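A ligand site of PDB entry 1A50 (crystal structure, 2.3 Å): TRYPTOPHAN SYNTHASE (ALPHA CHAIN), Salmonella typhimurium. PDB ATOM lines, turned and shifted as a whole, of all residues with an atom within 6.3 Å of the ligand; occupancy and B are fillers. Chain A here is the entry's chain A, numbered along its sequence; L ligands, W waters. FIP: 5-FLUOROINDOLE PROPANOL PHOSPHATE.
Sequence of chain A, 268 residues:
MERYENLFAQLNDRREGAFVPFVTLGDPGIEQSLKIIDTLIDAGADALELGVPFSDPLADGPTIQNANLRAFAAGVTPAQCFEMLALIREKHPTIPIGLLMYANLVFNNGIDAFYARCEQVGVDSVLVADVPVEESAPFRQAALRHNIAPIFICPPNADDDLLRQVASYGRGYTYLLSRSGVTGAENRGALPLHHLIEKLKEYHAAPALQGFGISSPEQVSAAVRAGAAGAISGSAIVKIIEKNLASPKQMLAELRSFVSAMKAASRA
Merely in contact with the ligand: Phe 22 (3.6 Å), Ala 59 (3.8 Å), Ile 64 (3.7 Å), Leu 100 (3.7 Å), Ala 129 (3.99 Å), Ile 153 (2.9 Å), Tyr 175 (2.9 Å), Thr 183 (3.4 Å), Phe 212 (3.2 Å) and Ser 233 (3.8 Å).
Hydrophobic or aromatic side chains that line the ligand: Phe 22, Ala 59, Ile 64, Leu 100, Ala 129, Ile 153, Tyr 175 and Phe 212.
Within 4 Å of the ligand: Phe 22, Ala 59, Asp 60, Ile 64, Leu 100, Ala 129, Ile 153, Tyr 175, Thr 183, Gly 184, Phe 212, Gly 213, Ser 233, Gly 234 and Ser 235.
The nearest printed residue that does not touch the ligand is Ile 232 (4.03 Å).
The side-chain hydroxyl (OG) of Ser 235 sits close to an oxygen (OP1) of the ligand.
N of Gly 234 lies close to OP2 of the ligand.
The backbone NH of Gly 184 lies close to an oxygen (OP3) of the ligand, 3.1 Å away.
A nitrogen (N1) of the ligand lies close to the side-chain carboxylate of Asp 60.
The backbone NH of Gly 213 lies close to an oxygen (OP3) of the ligand (2.8 Å).
The backbone NH (N) of Ser 235 sits close to an oxygen (OP1) of the ligand (2.7 Å).
The backbone NH (N) of Phe 22 lies within hydrogen-bond range of the backbone carbonyl oxygen (O) of Ser 233, 3.0 Å away.
The side-chain hydroxyl of Ser 233 sits at hydrogen-bond distance from the backbone carbonyl oxygen of Ile 214 (2.9 Å).
OG1 of Thr 183 is in hydrogen-bond range of OD1 of Asp 60 (3.2 Å).
NH2 of Arg 179 lies within hydrogen-bond range of O of Gly 184, 3.1 Å away.
OH of Tyr 102 is in hydrogen-bond range of N of Ala 59, 3.0 Å away.
O of Gly 213 is in hydrogen-bond range of OG of Ser 215, at 3.4 Å.
The side-chain carboxylate (OD2) of Asp 60 is in hydrogen-bond range of the side-chain hydroxyl (OH) of Tyr 102 (2.5 Å).
The backbone NH (N) of Thr 183 lies within hydrogen-bond range of the backbone carbonyl oxygen (O) of Ala 59, at 3.5 Å.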
ATOM      1  N   PHE A  22      20.242 -19.742   2.382  1.00  0.00           N
ATOM      2  CA  PHE A  22      20.091 -18.569   3.215  1.00  0.00           C
ATOM      3  C   PHE A  22      19.504 -17.469   2.341  1.00  0.00           C
ATOM      4  O   PHE A  22      19.943 -17.284   1.203  1.00  0.00           O
ATOM      5  CB  PHE A  22      21.436 -18.076   3.770  1.00  0.00           C
ATOM      6  CG  PHE A  22      21.407 -16.636   4.218  1.00  0.00           C
ATOM      7  CD1 PHE A  22      21.415 -15.605   3.286  1.00  0.00           C
ATOM      8  CD2 PHE A  22      21.275 -16.313   5.568  1.00  0.00           C
ATOM      9  CE1 PHE A  22      21.291 -14.289   3.688  1.00  0.00           C
ATOM     10  CE2 PHE A  22      21.151 -14.997   5.970  1.00  0.00           C
ATOM     11  CZ  PHE A  22      21.158 -13.985   5.037  1.00  0.00           C
ATOM     12  N   GLU A  49      18.279 -20.765   6.745  1.00  0.00           N
ATOM     13  CA  GLU A  49      19.108 -19.824   7.495  1.00  0.00           C
ATOM     14  C   GLU A  49      18.503 -18.503   7.022  1.00  0.00           C
ATOM     15  O   GLU A  49      18.532 -18.181   5.834  1.00  0.00           O
ATOM     16  CB  GLU A  49      20.582 -19.956   7.096  1.00  0.00           C
ATOM     17  CG  GLU A  49      21.545 -19.395   8.124  1.00  0.00           C
ATOM     18  CD  GLU A  49      21.306 -19.913   9.539  1.00  0.00           C
ATOM     19  OE1 GLU A  49      21.010 -21.113   9.703  1.00  0.00           O
ATOM     20  OE2 GLU A  49      21.419 -19.105  10.480  1.00  0.00           O
ATOM     21  N   ALA A  59      29.502  -8.143   8.155  1.00  0.00           N
ATOM     22  CA  ALA A  59      30.096  -9.443   7.870  1.00  0.00           C
ATOM     23  C   ALA A  59      29.548  -9.932   6.527  1.00  0.00           C
ATOM     24  O   ALA A  59      29.741 -11.081   6.144  1.00  0.00           O
ATOM     25  CB  ALA A  59      29.755 -10.450   8.957  1.00  0.00           C
ATOM     26  N   ASP A  60      28.874  -9.037   5.808  1.00  0.00           N
ATOM     27  CA  ASP A  60      28.257  -9.378   4.539  1.00  0.00           C
ATOM     28  C   ASP A  60      28.868  -8.733   3.299  1.00  0.00           C
ATOM     29  O   ASP A  60      29.302  -7.568   3.332  1.00  0.00           O
ATOM     30  CB  ASP A  60      26.766  -9.055   4.579  1.00  0.00           C
ATOM     31  CG  ASP A  60      25.958 -10.079   5.357  1.00  0.00           C
ATOM     32  OD1 ASP A  60      25.865 -11.243   4.881  1.00  0.00           O
ATOM     33  OD2 ASP A  60      25.429  -9.737   6.446  1.00  0.00           O
ATOM     34  N   ILE A  64      24.451  -9.734  -0.453  1.00  0.00           N
ATOM     35  CA  ILE A  64      23.553  -9.692   0.687  1.00  0.00           C
ATOM     36  C   ILE A  64      23.356  -8.270   1.218  1.00  0.00           C
ATOM     37  O   ILE A  64      22.312  -7.972   1.797  1.00  0.00           O
ATOM     38  CB  ILE A  64      24.056 -10.661   1.783  1.00  0.00           C
ATOM     39  CG1 ILE A  64      23.796 -12.100   1.327  1.00  0.00           C
ATOM     40  CG2 ILE A  64      23.321 -10.404   3.106  1.00  0.00           C
ATOM     41  CD1 ILE A  64      24.318 -13.150   2.250  1.00  0.00           C
ATOM     42  N   LEU A 100      20.165 -15.519  11.181  1.00  0.00           N
ATOM     43  CA  LEU A 100      21.490 -14.931  11.074  1.00  0.00           C
ATOM     44  C   LEU A 100      21.231 -13.505  11.566  1.00  0.00           C
ATOM     45  O   LEU A 100      20.551 -12.722  10.884  1.00  0.00           O
ATOM     46  CB  LEU A 100      21.980 -14.931   9.617  1.00  0.00           C
ATOM     47  CG  LEU A 100      23.469 -14.613   9.405  1.00  0.00           C
ATOM     48  CD1 LEU A 100      23.725 -13.155   9.692  1.00  0.00           C
ATOM     49  CD2 LEU A 100      24.319 -15.465  10.320  1.00  0.00           C
ATOM     50  N   TYR A 102      22.630  -9.764  13.745  1.00  0.00           N
ATOM     51  CA  TYR A 102      23.719  -8.850  14.082  1.00  0.00           C
ATOM     52  C   TYR A 102      23.338  -8.471  15.514  1.00  0.00           C
ATOM     53  O   TYR A 102      22.151  -8.334  15.829  1.00  0.00           O
ATOM     54  CB  TYR A 102      23.756  -7.658  13.139  1.00  0.00           C
ATOM     55  CG  TYR A 102      24.555  -7.982  11.901  1.00  0.00           C
ATOM     56  CD1 TYR A 102      25.947  -8.035  11.934  1.00  0.00           C
ATOM     57  CD2 TYR A 102      23.920  -8.317  10.717  1.00  0.00           C
ATOM     58  CE1 TYR A 102      26.681  -8.423  10.818  1.00  0.00           C
ATOM     59  CE2 TYR A 102      24.648  -8.704   9.593  1.00  0.00           C
ATOM     60  CZ  TYR A 102      26.017  -8.758   9.660  1.00  0.00           C
ATOM     61  OH  TYR A 102      26.715  -9.145   8.549  1.00  0.00           O
ATOM     62  N   LEU A 127      22.441 -17.348  15.153  1.00  0.00           N
ATOM     63  CA  LEU A 127      23.856 -17.108  14.947  1.00  0.00           C
ATOM     64  C   LEU A 127      24.000 -15.581  14.962  1.00  0.00           C
ATOM     65  O   LEU A 127      23.432 -14.893  14.104  1.00  0.00           O
ATOM     66  CB  LEU A 127      24.291 -17.672  13.586  1.00  0.00           C
ATOM     67  CG  LEU A 127      25.796 -17.782  13.296  1.00  0.00           C
ATOM     68  CD1 LEU A 127      26.010 -18.133  11.829  1.00  0.00           C
ATOM     69  CD2 LEU A 127      26.483 -16.462  13.626  1.00  0.00           C
ATOM     70  N   ALA A 129      26.292 -12.858  14.192  1.00  0.00           N
ATOM     71  CA  ALA A 129      27.528 -12.633  13.445  1.00  0.00           C
ATOM     72  C   ALA A 129      28.645 -11.837  14.110  1.00  0.00           C
ATOM     73  O   ALA A 129      29.816 -12.172  13.955  1.00  0.00           O
ATOM     74  CB  ALA A 129      27.172 -12.026  12.089  1.00  0.00           C
ATOM     75  N   ILE A 153      30.686 -19.669  15.074  1.00  0.00           N
ATOM     76  CA  ILE A 153      31.493 -19.764  13.862  1.00  0.00           C
ATOM     77  C   ILE A 153      32.897 -20.291  14.141  1.00  0.00           C
ATOM     78  O   ILE A 153      33.595 -19.803  15.025  1.00  0.00           O
ATOM     79  CB  ILE A 153      31.616 -18.380  13.181  1.00  0.00           C
ATOM     80  CG1 ILE A 153      30.249 -17.941  12.659  1.00  0.00           C
ATOM     81  CG2 ILE A 153      32.619 -18.455  12.038  1.00  0.00           C
ATOM     82  CD1 ILE A 153      30.306 -16.742  11.738  1.00  0.00           C
ATOM     83  N   TYR A 175      28.943 -23.615  12.647  1.00  0.00           N
ATOM     84  CA  TYR A 175      29.103 -22.951  11.371  1.00  0.00           C
ATOM     85  C   TYR A 175      30.591 -22.988  11.048  1.00  0.00           C
ATOM     86  O   TYR A 175      31.419 -22.456  11.777  1.00  0.00           O
ATOM     87  CB  TYR A 175      28.604 -21.512  11.419  1.00  0.00           C
ATOM     88  CG  TYR A 175      28.563 -20.838  10.069  1.00  0.00           C
ATOM     89  CD1 TYR A 175      29.676 -20.161   9.580  1.00  0.00           C
ATOM     90  CD2 TYR A 175      27.417 -20.855   9.294  1.00  0.00           C
ATOM     91  CE1 TYR A 175      29.642 -19.522   8.342  1.00  0.00           C
ATOM     92  CE2 TYR A 175      27.375 -20.226   8.062  1.00  0.00           C
ATOM     93  CZ  TYR A 175      28.494 -19.561   7.593  1.00  0.00           C
ATOM     94  OH  TYR A 175      28.473 -18.933   6.370  1.00  0.00           O
ATOM     95  N   LEU A 177      33.558 -21.906   8.633  1.00  0.00           N
ATOM     96  CA  LEU A 177      33.945 -20.914   7.626  1.00  0.00           C
ATOM     97  C   LEU A 177      34.926 -21.518   6.632  1.00  0.00           C
ATOM     98  O   LEU A 177      36.002 -21.979   7.011  1.00  0.00           O
ATOM     99  CB  LEU A 177      34.616 -19.723   8.311  1.00  0.00           C
ATOM    100  CG  LEU A 177      33.792 -18.469   8.489  1.00  0.00           C
ATOM    101  CD1 LEU A 177      34.684 -17.391   9.086  1.00  0.00           C
ATOM    102  CD2 LEU A 177      33.202 -18.036   7.155  1.00  0.00           C
ATOM    103  N   ARG A 179      36.475 -19.854   4.429  1.00  0.00           N
ATOM    104  CA  ARG A 179      37.524 -18.867   4.186  1.00  0.00           C
ATOM    105  C   ARG A 179      37.318 -17.633   5.047  1.00  0.00           C
ATOM    106  O   ARG A 179      36.317 -17.514   5.761  1.00  0.00           O
ATOM    107  CB  ARG A 179      37.479 -18.408   2.740  1.00  0.00           C
ATOM    108  CG  ARG A 179      36.163 -17.729   2.381  1.00  0.00           C
ATOM    109  CD  ARG A 179      36.154 -17.241   0.945  1.00  0.00           C
ATOM    110  NE  ARG A 179      34.831 -16.828   0.502  1.00  0.00           N
ATOM    111  CZ  ARG A 179      34.160 -15.789   1.010  1.00  0.00           C
ATOM    112  NH1 ARG A 179      34.687 -15.048   1.976  1.00  0.00           N
ATOM    113  NH2 ARG A 179      32.964 -15.488   0.510  1.00  0.00           N
ATOM    114  N   VAL A 182      34.290 -11.864   3.799  1.00  0.00           N
ATOM    115  CA  VAL A 182      32.851 -11.763   4.028  1.00  0.00           C
ATOM    116  C   VAL A 182      32.059 -12.688   3.111  1.00  0.00           C
ATOM    117  O   VAL A 182      32.642 -13.439   2.329  1.00  0.00           O
ATOM    118  CB  VAL A 182      32.358 -10.293   3.845  1.00  0.00           C
ATOM    119  CG1 VAL A 182      33.016  -9.379   4.869  1.00  0.00           C
ATOM    120  CG2 VAL A 182      32.659  -9.798   2.440  1.00  0.00           C
ATOM    121  N   THR A 183      30.738 -12.635   3.216  1.00  0.00           N
ATOM    122  CA  THR A 183      29.869 -13.460   2.377  1.00  0.00           C
ATOM    123  C   THR A 183      29.979 -13.055   0.908  1.00  0.00           C
ATOM    124  O   THR A 183      29.970 -11.875   0.585  1.00  0.00           O
ATOM    125  CB  THR A 183      28.377 -13.350   2.831  1.00  0.00           C
ATOM    126  OG1 THR A 183      27.889 -12.036   2.576  1.00  0.00           O
ATOM    127  CG2 THR A 183      28.256 -13.665   4.319  1.00  0.00           C
ATOM    128  N   GLY A 184      30.082 -14.044   0.026  1.00  0.00           N
ATOM    129  CA  GLY A 184      30.193 -13.752  -1.400  1.00  0.00           C
ATOM    130  C   GLY A 184      30.282 -15.024  -2.212  1.00  0.00           C
ATOM    131  O   GLY A 184      31.181 -15.851  -1.989  1.00  0.00           O
ATOM    132  N   ALA A 185      29.359 -15.180  -3.161  1.00  0.00           N
ATOM    133  CA  ALA A 185      29.312 -16.365  -4.019  1.00  0.00           C
ATOM    134  C   ALA A 185      30.535 -16.482  -4.919  1.00  0.00           C
ATOM    135  O   ALA A 185      31.102 -17.567  -5.066  1.00  0.00           O
ATOM    136  CB  ALA A 185      28.043 -16.355  -4.856  1.00  0.00           C
ATOM    137  N   GLY A 211      30.062 -22.904   5.318  1.00  0.00           N
ATOM    138  CA  GLY A 211      29.460 -21.764   4.651  1.00  0.00           C
ATOM    139  C   GLY A 211      30.468 -20.750   4.124  1.00  0.00           C
ATOM    140  O   GLY A 211      31.610 -20.676   4.584  1.00  0.00           O
ATOM    141  N   PHE A 212      30.015 -19.961   3.156  1.00  0.00           N
ATOM    142  CA  PHE A 212      30.805 -18.912   2.492  1.00  0.00           C
ATOM    143  C   PHE A 212      31.314 -19.369   1.140  1.00  0.00           C
ATOM    144  O   PHE A 212      32.170 -20.238   1.047  1.00  0.00           O
ATOM    145  CB  PHE A 212      31.984 -18.460   3.356  1.00  0.00           C
ATOM    146  CG  PHE A 212      31.706 -17.252   4.198  1.00  0.00           C
ATOM    147  CD1 PHE A 212      30.419 -16.989   4.656  1.00  0.00           C
ATOM    148  CD2 PHE A 212      32.729 -16.377   4.565  1.00  0.00           C
ATOM    149  CE1 PHE A 212      30.153 -15.880   5.465  1.00  0.00           C
ATOM    150  CE2 PHE A 212      32.477 -15.279   5.374  1.00  0.00           C
ATOM    151  CZ  PHE A 212      31.196 -15.026   5.825  1.00  0.00           C
ATOM    152  N   GLY A 213      30.773 -18.792   0.072  1.00  0.00           N
ATOM    153  CA  GLY A 213      31.215 -19.137  -1.263  1.00  0.00           C
ATOM    154  C   GLY A 213      30.645 -20.375  -1.909  1.00  0.00           C
ATOM    155  O   GLY A 213      30.920 -20.623  -3.085  1.00  0.00           O
ATOM    156  N   ILE A 214      29.856 -21.166  -1.182  1.00  0.00           N
ATOM    157  CA  ILE A 214      29.262 -22.377  -1.750  1.00  0.00           C
ATOM    158  C   ILE A 214      28.210 -22.002  -2.806  1.00  0.00           C
ATOM    159  O   ILE A 214      27.104 -21.588  -2.472  1.00  0.00           O
ATOM    160  CB  ILE A 214      28.573 -23.222  -0.659  1.00  0.00           C
ATOM    161  CG1 ILE A 214      29.540 -23.470   0.512  1.00  0.00           C
ATOM    162  CG2 ILE A 214      28.091 -24.525  -1.254  1.00  0.00           C
ATOM    163  CD1 ILE A 214      30.551 -24.546   0.275  1.00  0.00           C
ATOM    164  N   SER A 215      28.571 -22.157  -4.078  1.00  0.00           N
ATOM    165  CA  SER A 215      27.653 -21.815  -5.164  1.00  0.00           C
ATOM    166  C   SER A 215      27.465 -22.894  -6.222  1.00  0.00           C
ATOM    167  O   SER A 215      26.560 -22.807  -7.058  1.00  0.00           O
ATOM    168  CB  SER A 215      28.141 -20.534  -5.846  1.00  0.00           C
ATOM    169  OG  SER A 215      29.508 -20.654  -6.229  1.00  0.00           O
ATOM    170  N   ILE A 232      25.957 -24.483   3.558  1.00  0.00           N
ATOM    171  CA  ILE A 232      25.045 -23.357   3.548  1.00  0.00           C
ATOM    172  C   ILE A 232      25.400 -22.523   2.326  1.00  0.00           C
ATOM    173  O   ILE A 232      26.577 -22.320   2.036  1.00  0.00           O
ATOM    174  CB  ILE A 232      25.201 -22.478   4.807  1.00  0.00           C
ATOM    175  CG1 ILE A 232      24.658 -23.225   6.031  1.00  0.00           C
ATOM    176  CG2 ILE A 232      24.432 -21.168   4.629  1.00  0.00           C
ATOM    177  CD1 ILE A 232      25.162 -22.652   7.341  1.00  0.00           C
ATOM    178  N   SER A 233      24.398 -22.048   1.612  1.00  0.00           N
ATOM    179  CA  SER A 233      24.644 -21.232   0.433  1.00  0.00           C
ATOM    180  C   SER A 233      23.711 -20.028   0.475  1.00  0.00           C
ATOM    181  O   SER A 233      22.498 -20.187   0.532  1.00  0.00           O
ATOM    182  CB  SER A 233      24.397 -22.068  -0.835  1.00  0.00           C
ATOM    183  OG  SER A 233      24.302 -21.261  -1.990  1.00  0.00           O
ATOM    184  N   GLY A 234      24.277 -18.825   0.446  1.00  0.00           N
ATOM    185  CA  GLY A 234      23.458 -17.615   0.494  1.00  0.00           C
ATOM    186  C   GLY A 234      23.518 -16.691  -0.710  1.00  0.00           C
ATOM    187  O   GLY A 234      22.517 -16.556  -1.428  1.00  0.00           O
ATOM    188  N   SER A 235      24.674 -16.059  -0.944  1.00  0.00           N
ATOM    189  CA  SER A 235      24.823 -15.132  -2.080  1.00  0.00           C
ATOM    190  C   SER A 235      24.410 -15.768  -3.410  1.00  0.00           C
ATOM    191  O   SER A 235      23.819 -15.099  -4.264  1.00  0.00           O
ATOM    192  CB  SER A 235      26.271 -14.648  -2.186  1.00  0.00           C
ATOM    193  OG  SER A 235      26.691 -13.996  -0.997  1.00  0.00           O
ATOM    194  N   ALA A 236      24.722 -17.053  -3.574  1.00  0.00           N
ATOM    195  CA  ALA A 236      24.380 -17.756  -4.811  1.00  0.00           C
ATOM    196  C   ALA A 236      22.870 -17.812  -4.991  1.00  0.00           C
ATOM    197  O   ALA A 236      22.361 -17.744  -6.105  1.00  0.00           O
ATOM    198  CB  ALA A 236      24.961 -19.162  -4.783  1.00  0.00           C
HETATM  199  C3  FIP L   1      25.433 -15.796   5.999  1.00  0.00           C
HETATM  200  C9  FIP L   1      26.411 -15.330   6.924  1.00  0.00           C
HETATM  201  C8  FIP L   1      26.263 -13.928   7.032  1.00  0.00           C
HETATM  202  C4  FIP L   1      27.397 -15.958   7.694  1.00  0.00           C
HETATM  203  C2  FIP L   1      24.760 -14.696   5.568  1.00  0.00           C
HETATM  204  N1  FIP L   1      25.242 -13.565   6.190  1.00  0.00           N
HETATM  205  C7  FIP L   1      27.060 -13.149   7.864  1.00  0.00           C
HETATM  206  C5  FIP L   1      28.187 -15.180   8.533  1.00  0.00           C
HETATM  207  C6  FIP L   1      28.011 -13.785   8.610  1.00  0.00           C
HETATM  208  F   FIP L   1      29.125 -15.776   9.295  1.00  0.00           F
HETATM  209  C3P FIP L   1      25.222 -17.208   5.569  1.00  0.00           C
HETATM  210  C2P FIP L   1      26.401 -17.657   4.720  1.00  0.00           C
HETATM  211  C1P FIP L   1      26.345 -16.991   3.354  1.00  0.00           C
HETATM  212  P   FIP L   1      27.609 -16.963   1.024  1.00  0.00           P
HETATM  213  OP1 FIP L   1      26.739 -15.767   0.807  1.00  0.00           O
HETATM  214  OP2 FIP L   1      27.029 -18.178   0.337  1.00  0.00           O
HETATM  215  OP3 FIP L   1      29.065 -16.791   0.938  1.00  0.00           O
HETATM  216  OP4 FIP L   1      27.466 -17.372   2.591  1.00  0.00           O
HETATM  217  O   HOH W   1      28.438 -20.364   0.899  1.00  0.00           O
HETATM  218  O   HOH W   2      26.424 -18.667  -2.293  1.00  0.00           O
